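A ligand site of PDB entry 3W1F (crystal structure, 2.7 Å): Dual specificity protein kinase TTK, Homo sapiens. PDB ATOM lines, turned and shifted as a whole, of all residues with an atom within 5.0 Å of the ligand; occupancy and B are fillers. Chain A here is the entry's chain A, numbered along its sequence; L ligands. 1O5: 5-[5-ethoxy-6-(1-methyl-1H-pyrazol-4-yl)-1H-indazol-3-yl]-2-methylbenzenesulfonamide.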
ATOM      1  N   LYS A  15     -25.117  13.769  11.144  1.00  0.00           N
ATOM      2  CA  LYS A  15     -25.302  12.347  10.774  1.00  0.00           C
ATOM      3  C   LYS A  15     -24.082  11.763  10.054  1.00  0.00           C
ATOM      4  O   LYS A  15     -23.414  12.447   9.287  1.00  0.00           O
ATOM      5  CB  LYS A  15     -26.529  12.197   9.869  1.00  0.00           C
ATOM      6  CG  LYS A  15     -26.672  10.861   9.192  1.00  0.00           C
ATOM      7  CD  LYS A  15     -27.919  10.838   8.335  1.00  0.00           C
ATOM      8  CE  LYS A  15     -27.672  11.366   6.961  1.00  0.00           C
ATOM      9  NZ  LYS A  15     -28.708  10.824   6.035  1.00  0.00           N
ATOM     10  N   ILE A  17     -22.723   9.396   7.162  1.00  0.00           N
ATOM     11  CA  ILE A  17     -23.219   8.878   5.896  1.00  0.00           C
ATOM     12  C   ILE A  17     -22.348   7.766   5.322  1.00  0.00           C
ATOM     13  O   ILE A  17     -22.845   6.895   4.622  1.00  0.00           O
ATOM     14  CB  ILE A  17     -23.437   9.975   4.848  1.00  0.00           C
ATOM     15  CG1 ILE A  17     -22.311  11.006   4.886  1.00  0.00           C
ATOM     16  CG2 ILE A  17     -24.699  10.675   5.135  1.00  0.00           C
ATOM     17  CD1 ILE A  17     -22.641  12.329   4.165  1.00  0.00           C
ATOM     18  N   GLY A  18     -21.054   7.804   5.639  1.00  0.00           N
ATOM     19  CA  GLY A  18     -20.087   6.884   5.044  1.00  0.00           C
ATOM     20  C   GLY A  18     -19.059   6.412   6.055  1.00  0.00           C
ATOM     21  O   GLY A  18     -18.856   7.056   7.103  1.00  0.00           O
ATOM     22  N   VAL A  25     -17.458   9.611   6.677  1.00  0.00           N
ATOM     23  CA  VAL A  25     -18.070  10.803   6.087  1.00  0.00           C
ATOM     24  C   VAL A  25     -19.275  11.265   6.908  1.00  0.00           C
ATOM     25  O   VAL A  25     -20.171  10.465   7.209  1.00  0.00           O
ATOM     26  CB  VAL A  25     -18.534  10.581   4.633  1.00  0.00           C
ATOM     27  CG1 VAL A  25     -18.593  11.926   3.866  1.00  0.00           C
ATOM     28  CG2 VAL A  25     -17.648   9.580   3.932  1.00  0.00           C
ATOM     29  N   GLN A  27     -22.480  14.122   7.330  1.00  0.00           N
ATOM     30  CA  GLN A  27     -23.379  15.169   6.900  1.00  0.00           C
ATOM     31  C   GLN A  27     -23.304  16.217   8.006  1.00  0.00           C
ATOM     32  O   GLN A  27     -23.613  15.908   9.165  1.00  0.00           O
ATOM     33  CB  GLN A  27     -24.772  14.573   6.777  1.00  0.00           C
ATOM     34  CG  GLN A  27     -25.783  15.411   6.054  1.00  0.00           C
ATOM     35  CD  GLN A  27     -27.204  14.913   6.300  1.00  0.00           C
ATOM     36  OE1 GLN A  27     -27.574  14.615   7.433  1.00  0.00           O
ATOM     37  NE2 GLN A  27     -28.006  14.847   5.246  1.00  0.00           N
ATOM     38  N   ILE A  35     -25.295  23.000   4.555  1.00  0.00           N
ATOM     39  CA  ILE A  35     -24.877  21.617   4.593  1.00  0.00           C
ATOM     40  C   ILE A  35     -23.572  21.384   3.787  1.00  0.00           C
ATOM     41  O   ILE A  35     -23.220  22.162   2.885  1.00  0.00           O
ATOM     42  CB  ILE A  35     -26.025  20.626   4.194  1.00  0.00           C
ATOM     43  CG1 ILE A  35     -25.915  19.325   4.985  1.00  0.00           C
ATOM     44  CG2 ILE A  35     -26.044  20.382   2.676  1.00  0.00           C
ATOM     45  CD1 ILE A  35     -27.007  18.322   4.656  1.00  0.00           C
ATOM     46  N   ALA A  37     -20.637  17.797   3.214  1.00  0.00           N
ATOM     47  CA  ALA A  37     -20.117  16.514   3.629  1.00  0.00           C
ATOM     48  C   ALA A  37     -18.687  16.773   4.036  1.00  0.00           C
ATOM     49  O   ALA A  37     -17.980  17.548   3.370  1.00  0.00           O
ATOM     50  CB  ALA A  37     -20.192  15.526   2.512  1.00  0.00           C
ATOM     51  N   LYS A  39     -15.204  14.626   5.101  1.00  0.00           N
ATOM     52  CA  LYS A  39     -14.550  13.342   5.257  1.00  0.00           C
ATOM     53  C   LYS A  39     -13.425  13.409   6.272  1.00  0.00           C
ATOM     54  O   LYS A  39     -12.491  14.185   6.136  1.00  0.00           O
ATOM     55  CB  LYS A  39     -14.081  12.811   3.903  1.00  0.00           C
ATOM     56  CG  LYS A  39     -13.310  11.497   3.985  1.00  0.00           C
ATOM     57  CD  LYS A  39     -13.420  10.768   2.684  1.00  0.00           C
ATOM     58  CE  LYS A  39     -12.073  10.339   2.138  1.00  0.00           C
ATOM     59  NZ  LYS A  39     -12.231   9.994   0.695  1.00  0.00           N
ATOM     60  N   GLU A  57      -5.261  11.446  -4.064  1.00  0.00           N
ATOM     61  CA  GLU A  57      -6.689  11.725  -4.230  1.00  0.00           C
ATOM     62  C   GLU A  57      -6.984  13.212  -4.028  1.00  0.00           C
ATOM     63  O   GLU A  57      -7.531  13.840  -4.918  1.00  0.00           O
ATOM     64  CB  GLU A  57      -7.522  10.874  -3.262  1.00  0.00           C
ATOM     65  CG  GLU A  57      -9.051  11.034  -3.412  1.00  0.00           C
ATOM     66  CD  GLU A  57      -9.864  10.665  -2.140  1.00  0.00           C
ATOM     67  OE1 GLU A  57      -9.462  11.026  -1.010  1.00  0.00           O
ATOM     68  OE2 GLU A  57     -10.930  10.018  -2.294  1.00  0.00           O
ATOM     69  N   LEU A  61      -8.320  15.623  -6.861  1.00  0.00           N
ATOM     70  CA  LEU A  61      -9.662  16.090  -6.580  1.00  0.00           C
ATOM     71  C   LEU A  61      -9.649  17.592  -6.666  1.00  0.00           C
ATOM     72  O   LEU A  61     -10.515  18.172  -7.299  1.00  0.00           O
ATOM     73  CB  LEU A  61     -10.113  15.589  -5.214  1.00  0.00           C
ATOM     74  CG  LEU A  61     -11.539  15.946  -4.839  1.00  0.00           C
ATOM     75  CD1 LEU A  61     -12.496  15.556  -5.931  1.00  0.00           C
ATOM     76  CD2 LEU A  61     -11.862  15.281  -3.524  1.00  0.00           C
ATOM     77  N   ILE A  72     -17.378  15.956  -7.735  1.00  0.00           N
ATOM     78  CA  ILE A  72     -17.589  16.437  -6.379  1.00  0.00           C
ATOM     79  C   ILE A  72     -16.707  17.661  -6.087  1.00  0.00           C
ATOM     80  O   ILE A  72     -15.518  17.671  -6.403  1.00  0.00           O
ATOM     81  CB  ILE A  72     -17.395  15.307  -5.312  1.00  0.00           C
ATOM     82  CG1 ILE A  72     -17.872  15.780  -3.941  1.00  0.00           C
ATOM     83  CG2 ILE A  72     -15.956  14.845  -5.229  1.00  0.00           C
ATOM     84  CD1 ILE A  72     -19.374  15.811  -3.829  1.00  0.00           C
ATOM     85  N   MET A  86     -11.860  16.747   4.840  1.00  0.00           N
ATOM     86  CA  MET A  86     -12.180  17.276   3.541  1.00  0.00           C
ATOM     87  C   MET A  86     -13.585  17.872   3.565  1.00  0.00           C
ATOM     88  O   MET A  86     -14.576  17.144   3.726  1.00  0.00           O
ATOM     89  CB  MET A  86     -12.077  16.188   2.453  1.00  0.00           C
ATOM     90  CG  MET A  86     -10.673  15.633   2.234  1.00  0.00           C
ATOM     91  SD  MET A  86     -10.663  14.413   0.904  1.00  0.00           S
ATOM     92  CE  MET A  86      -9.710  13.157   1.727  1.00  0.00           C
ATOM     93  N   MET A  88     -16.590  19.124   1.665  1.00  0.00           N
ATOM     94  CA  MET A  88     -17.088  18.855   0.319  1.00  0.00           C
ATOM     95  C   MET A  88     -18.581  19.049   0.179  1.00  0.00           C
ATOM     96  O   MET A  88     -19.320  19.095   1.165  1.00  0.00           O
ATOM     97  CB  MET A  88     -16.775  17.406  -0.069  1.00  0.00           C
ATOM     98  CG  MET A  88     -15.329  17.067  -0.237  1.00  0.00           C
ATOM     99  SD  MET A  88     -15.261  15.321  -0.571  1.00  0.00           S
ATOM    100  CE  MET A  88     -15.178  14.655   1.070  1.00  0.00           C
ATOM    101  N   GLU A  89     -19.024  19.149  -1.057  1.00  0.00           N
ATOM    102  CA  GLU A  89     -20.406  19.246  -1.439  1.00  0.00           C
ATOM    103  C   GLU A  89     -21.248  18.082  -0.870  1.00  0.00           C
ATOM    104  O   GLU A  89     -20.752  16.953  -0.757  1.00  0.00           O
ATOM    105  CB  GLU A  89     -20.439  19.204  -2.951  1.00  0.00           C
ATOM    106  CG  GLU A  89     -21.474  20.009  -3.656  1.00  0.00           C
ATOM    107  CD  GLU A  89     -21.359  19.819  -5.155  1.00  0.00           C
ATOM    108  OE1 GLU A  89     -20.406  19.136  -5.599  1.00  0.00           O
ATOM    109  OE2 GLU A  89     -22.225  20.319  -5.896  1.00  0.00           O
ATOM    110  N   CYS A  90     -22.499  18.364  -0.515  1.00  0.00           N
ATOM    111  CA  CYS A  90     -23.447  17.347  -0.021  1.00  0.00           C
ATOM    112  C   CYS A  90     -24.522  17.004  -1.063  1.00  0.00           C
ATOM    113  O   CYS A  90     -25.087  17.898  -1.692  1.00  0.00           O
ATOM    114  CB  CYS A  90     -24.133  17.796   1.278  1.00  0.00           C
ATOM    115  SG  CYS A  90     -24.751  16.454   2.359  1.00  0.00           S
ATOM    116  N   GLY A  91     -24.797  15.720  -1.232  1.00  0.00           N
ATOM    117  CA  GLY A  91     -25.824  15.279  -2.160  1.00  0.00           C
ATOM    118  C   GLY A  91     -26.991  14.559  -1.508  1.00  0.00           C
ATOM    119  O   GLY A  91     -27.069  14.434  -0.289  1.00  0.00           O
ATOM    120  N   ASN A  92     -27.903  14.085  -2.352  1.00  0.00           N
ATOM    121  CA  ASN A  92     -29.133  13.450  -1.906  1.00  0.00           C
ATOM    122  C   ASN A  92     -28.915  11.989  -1.620  1.00  0.00           C
ATOM    123  O   ASN A  92     -29.289  11.513  -0.557  1.00  0.00           O
ATOM    124  CB  ASN A  92     -30.231  13.588  -2.963  1.00  0.00           C
ATOM    125  CG  ASN A  92     -30.458  15.038  -3.398  1.00  0.00           C
ATOM    126  OD1 ASN A  92     -29.534  15.876  -3.365  1.00  0.00           O
ATOM    127  ND2 ASN A  92     -31.684  15.330  -3.827  1.00  0.00           N
ATOM    128  N   ILE A  93     -28.320  11.275  -2.575  1.00  0.00           N
ATOM    129  CA  ILE A  93     -28.088   9.815  -2.447  1.00  0.00           C
ATOM    130  C   ILE A  93     -27.037   9.312  -3.428  1.00  0.00           C
ATOM    131  O   ILE A  93     -26.982   9.756  -4.575  1.00  0.00           O
ATOM    132  CB  ILE A  93     -29.422   8.983  -2.590  1.00  0.00           C
ATOM    133  CG1 ILE A  93     -29.241   7.546  -2.087  1.00  0.00           C
ATOM    134  CG2 ILE A  93     -29.948   9.035  -4.045  1.00  0.00           C
ATOM    135  CD1 ILE A  93     -30.493   6.715  -2.103  1.00  0.00           C
ATOM    136  N   ASP A  94     -26.202   8.374  -2.992  1.00  0.00           N
ATOM    137  CA  ASP A  94     -25.349   7.703  -3.954  1.00  0.00           C
ATOM    138  C   ASP A  94     -26.248   6.963  -4.938  1.00  0.00           C
ATOM    139  O   ASP A  94     -27.363   6.575  -4.593  1.00  0.00           O
ATOM    140  CB  ASP A  94     -24.353   6.746  -3.276  1.00  0.00           C
ATOM    141  CG  ASP A  94     -25.018   5.549  -2.648  1.00  0.00           C
ATOM    142  OD1 ASP A  94     -24.907   4.432  -3.206  1.00  0.00           O
ATOM    143  OD2 ASP A  94     -25.652   5.738  -1.587  1.00  0.00           O
ATOM    144  N   LEU A 140     -22.863  10.390  -7.263  1.00  0.00           N
ATOM    145  CA  LEU A 140     -23.631  11.012  -6.229  1.00  0.00           C
ATOM    146  C   LEU A 140     -24.559  12.046  -6.846  1.00  0.00           C
ATOM    147  O   LEU A 140     -24.090  12.960  -7.514  1.00  0.00           O
ATOM    148  CB  LEU A 140     -22.683  11.677  -5.251  1.00  0.00           C
ATOM    149  CG  LEU A 140     -23.243  12.571  -4.161  1.00  0.00           C
ATOM    150  CD1 LEU A 140     -23.495  11.728  -2.940  1.00  0.00           C
ATOM    151  CD2 LEU A 140     -22.290  13.728  -3.853  1.00  0.00           C
ATOM    152  N   ILE A 149     -17.415  10.945  -7.129  1.00  0.00           N
ATOM    153  CA  ILE A 149     -16.978  11.047  -5.749  1.00  0.00           C
ATOM    154  C   ILE A 149     -15.505  10.718  -5.637  1.00  0.00           C
ATOM    155  O   ILE A 149     -14.782  11.402  -4.927  1.00  0.00           O
ATOM    156  CB  ILE A 149     -17.803  10.099  -4.857  1.00  0.00           C
ATOM    157  CG1 ILE A 149     -19.106  10.766  -4.444  1.00  0.00           C
ATOM    158  CG2 ILE A 149     -17.042   9.648  -3.591  1.00  0.00           C
ATOM    159  CD1 ILE A 149     -19.937   9.861  -3.546  1.00  0.00           C
ATOM    160  N   MET A 157     -14.433   3.787   0.026  1.00  0.00           N
ATOM    161  CA  MET A 157     -15.358   3.913   1.174  1.00  0.00           C
ATOM    162  C   MET A 157     -16.752   3.373   0.818  1.00  0.00           C
ATOM    163  O   MET A 157     -17.237   3.564  -0.300  1.00  0.00           O
ATOM    164  CB  MET A 157     -15.472   5.382   1.655  1.00  0.00           C
ATOM    165  CG  MET A 157     -14.217   5.972   2.304  1.00  0.00           C
ATOM    166  SD  MET A 157     -13.075   6.791   1.137  1.00  0.00           S
ATOM    167  CE  MET A 157     -11.509   6.721   2.020  1.00  0.00           C
ATOM    168  N   GLN A 158     -17.398   2.705   1.778  1.00  0.00           N
ATOM    169  CA  GLN A 158     -18.765   2.195   1.584  1.00  0.00           C
ATOM    170  C   GLN A 158     -19.790   3.095   2.294  1.00  0.00           C
ATOM    171  O   GLN A 158     -19.656   3.335   3.504  1.00  0.00           O
ATOM    172  CB  GLN A 158     -18.878   0.739   2.059  1.00  0.00           C
ATOM    173  N   PRO A 159     -20.813   3.609   1.542  1.00  0.00           N
ATOM    174  CA  PRO A 159     -21.834   4.526   2.106  1.00  0.00           C
ATOM    175  C   PRO A 159     -22.913   3.843   2.987  1.00  0.00           C
ATOM    176  O   PRO A 159     -23.444   2.796   2.625  1.00  0.00           O
ATOM    177  CB  PRO A 159     -22.473   5.180   0.861  1.00  0.00           C
ATOM    178  CG  PRO A 159     -21.592   4.779  -0.313  1.00  0.00           C
ATOM    179  CD  PRO A 159     -20.971   3.480   0.082  1.00  0.00           C
HETATM  180  O3  1O5 L   1     -27.227  11.945   3.776  1.00  0.00           O
HETATM  181  S   1O5 L   1     -27.123  12.629   2.517  1.00  0.00           S
HETATM  182  O2  1O5 L   1     -26.800  14.040   2.701  1.00  0.00           O
HETATM  183  N3  1O5 L   1     -28.536  12.616   1.735  1.00  0.00           N
HETATM  184  C12 1O5 L   1     -26.019  11.805   1.689  1.00  0.00           C
HETATM  185  C11 1O5 L   1     -24.872  12.492   1.314  1.00  0.00           C
HETATM  186  C13 1O5 L   1     -26.160  10.352   1.320  1.00  0.00           C
HETATM  187  C14 1O5 L   1     -27.353   9.517   1.675  1.00  0.00           C
HETATM  188  C15 1O5 L   1     -25.129   9.743   0.615  1.00  0.00           C
HETATM  189  C16 1O5 L   1     -24.007  10.492   0.265  1.00  0.00           C
HETATM  190  C10 1O5 L   1     -23.873  11.838   0.609  1.00  0.00           C
HETATM  191  C7  1O5 L   1     -22.673  12.640   0.246  1.00  0.00           C
HETATM  192  N2  1O5 L   1     -22.624  13.970  -0.009  1.00  0.00           N
HETATM  193  N1  1O5 L   1     -21.301  14.370  -0.294  1.00  0.00           N
HETATM  194  C8  1O5 L   1     -21.286  12.146   0.123  1.00  0.00           C
HETATM  195  C9  1O5 L   1     -20.742  10.886   0.269  1.00  0.00           C
HETATM  196  C3  1O5 L   1     -19.383  10.729   0.064  1.00  0.00           C
HETATM  197  O1  1O5 L   1     -18.794   9.496   0.186  1.00  0.00           O
HETATM  198  C2  1O5 L   1     -19.567   8.333   0.486  1.00  0.00           C
HETATM  199  C1  1O5 L   1     -18.594   7.310   1.038  1.00  0.00           C
HETATM  200  C6  1O5 L   1     -20.476  13.321  -0.234  1.00  0.00           C
HETATM  201  C5  1O5 L   1     -19.111  13.164  -0.432  1.00  0.00           C
HETATM  202  C4  1O5 L   1     -18.530  11.907  -0.277  1.00  0.00           C
HETATM  203  C17 1O5 L   1     -17.077  11.733  -0.510  1.00  0.00           C
HETATM  204  C20 1O5 L   1     -16.243  10.805   0.111  1.00  0.00           C
HETATM  205  N5  1O5 L   1     -15.004  10.959  -0.401  1.00  0.00           N
HETATM  206  N4  1O5 L   1     -15.091  11.968  -1.354  1.00  0.00           N
HETATM  207  C19 1O5 L   1     -13.830  12.305  -2.049  1.00  0.00           C
HETATM  208  C18 1O5 L   1     -16.328  12.455  -1.438  1.00  0.00           C
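The side-chain sulfur (SD) of Met 88 sits close to a nitrogen (N4) of the ligand. Merely in contact with the ligand: Ile 17, Ile 149, Ala 37, Leu 140, Glu 57, Met 157, Val 25 and Leu 61. Hydrophobic or aromatic side chains within 4 Å of the ligand: Ile 17, Val 25, Ala 37, Leu 61, Met 88, Leu 140, Ile 149 and Met 157. Within 4 Å of the ligand: Lys 15, Ile 17, Val 25, Gln 27, Ala 37, Lys 39, Glu 57, Leu 61, Met 88, Glu 89, Cys 90, Gly 91, Asn 92, Leu 140, Ile 149 and Met 157. The nearest printed residue that does not touch the ligand is Asp 94 (4.004 Å).
The backbone carbonyl oxygen of Asn 92 sits at hydrogen-bond distance from a nitrogen (N3) of the ligand (2.7 Å). The backbone carbonyl oxygen of Glu 89 is in hydrogen-bond range of a nitrogen (N1) of the ligand (2.7 Å). NZ of Lys 15 is in hydrogen-bond range of O3 of the ligand, 2.9 Å away. NE2 of Gln 27 sits at hydrogen-bond distance from O2 of the ligand. A nitrogen (N2) of the ligand lies within hydrogen-bond range of the backbone NH of Gly 91 (3.0 Å). N3 of the ligand lies within hydrogen-bond range of O of Gly 91 (3.1 Å). The side-chain amino group (NZ) of Lys 39 is in hydrogen-bond range of a nitrogen (N5) of the ligand (3.1 Å). SG of Cys 90 sits at hydrogen-bond distance from O2 of the ligand (3.2 Å).
The backbone carbonyl oxygen (O) of Lys 15 sits at hydrogen-bond distance from the backbone NH (N) of Gln 27 (2.7 Å). The side-chain amino group (NZ) of Lys 39 lies within salt-bridge range of the side-chain carboxylate (OE2) of Glu 57 (3.3 Å). The side-chain amino group of Lys 39 is in hydrogen-bond range of the side-chain sulfur of Met 157 (3.3 Å). The backbone NH (N) of Lys 39 lies within hydrogen-bond range of the backbone carbonyl oxygen (O) of Met 86 (2.9 Å). The backbone NH (N) of Ile 17 lies within hydrogen-bond range of the backbone carbonyl oxygen (O) of Val 25, at 2.8 Å. N of Met 88 is in hydrogen-bond range of O of Ala 37 (2.7 Å). The backbone carbonyl oxygen of Gly 18 is in hydrogen-bond range of the backbone NH of Val 25 (2.9 Å).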
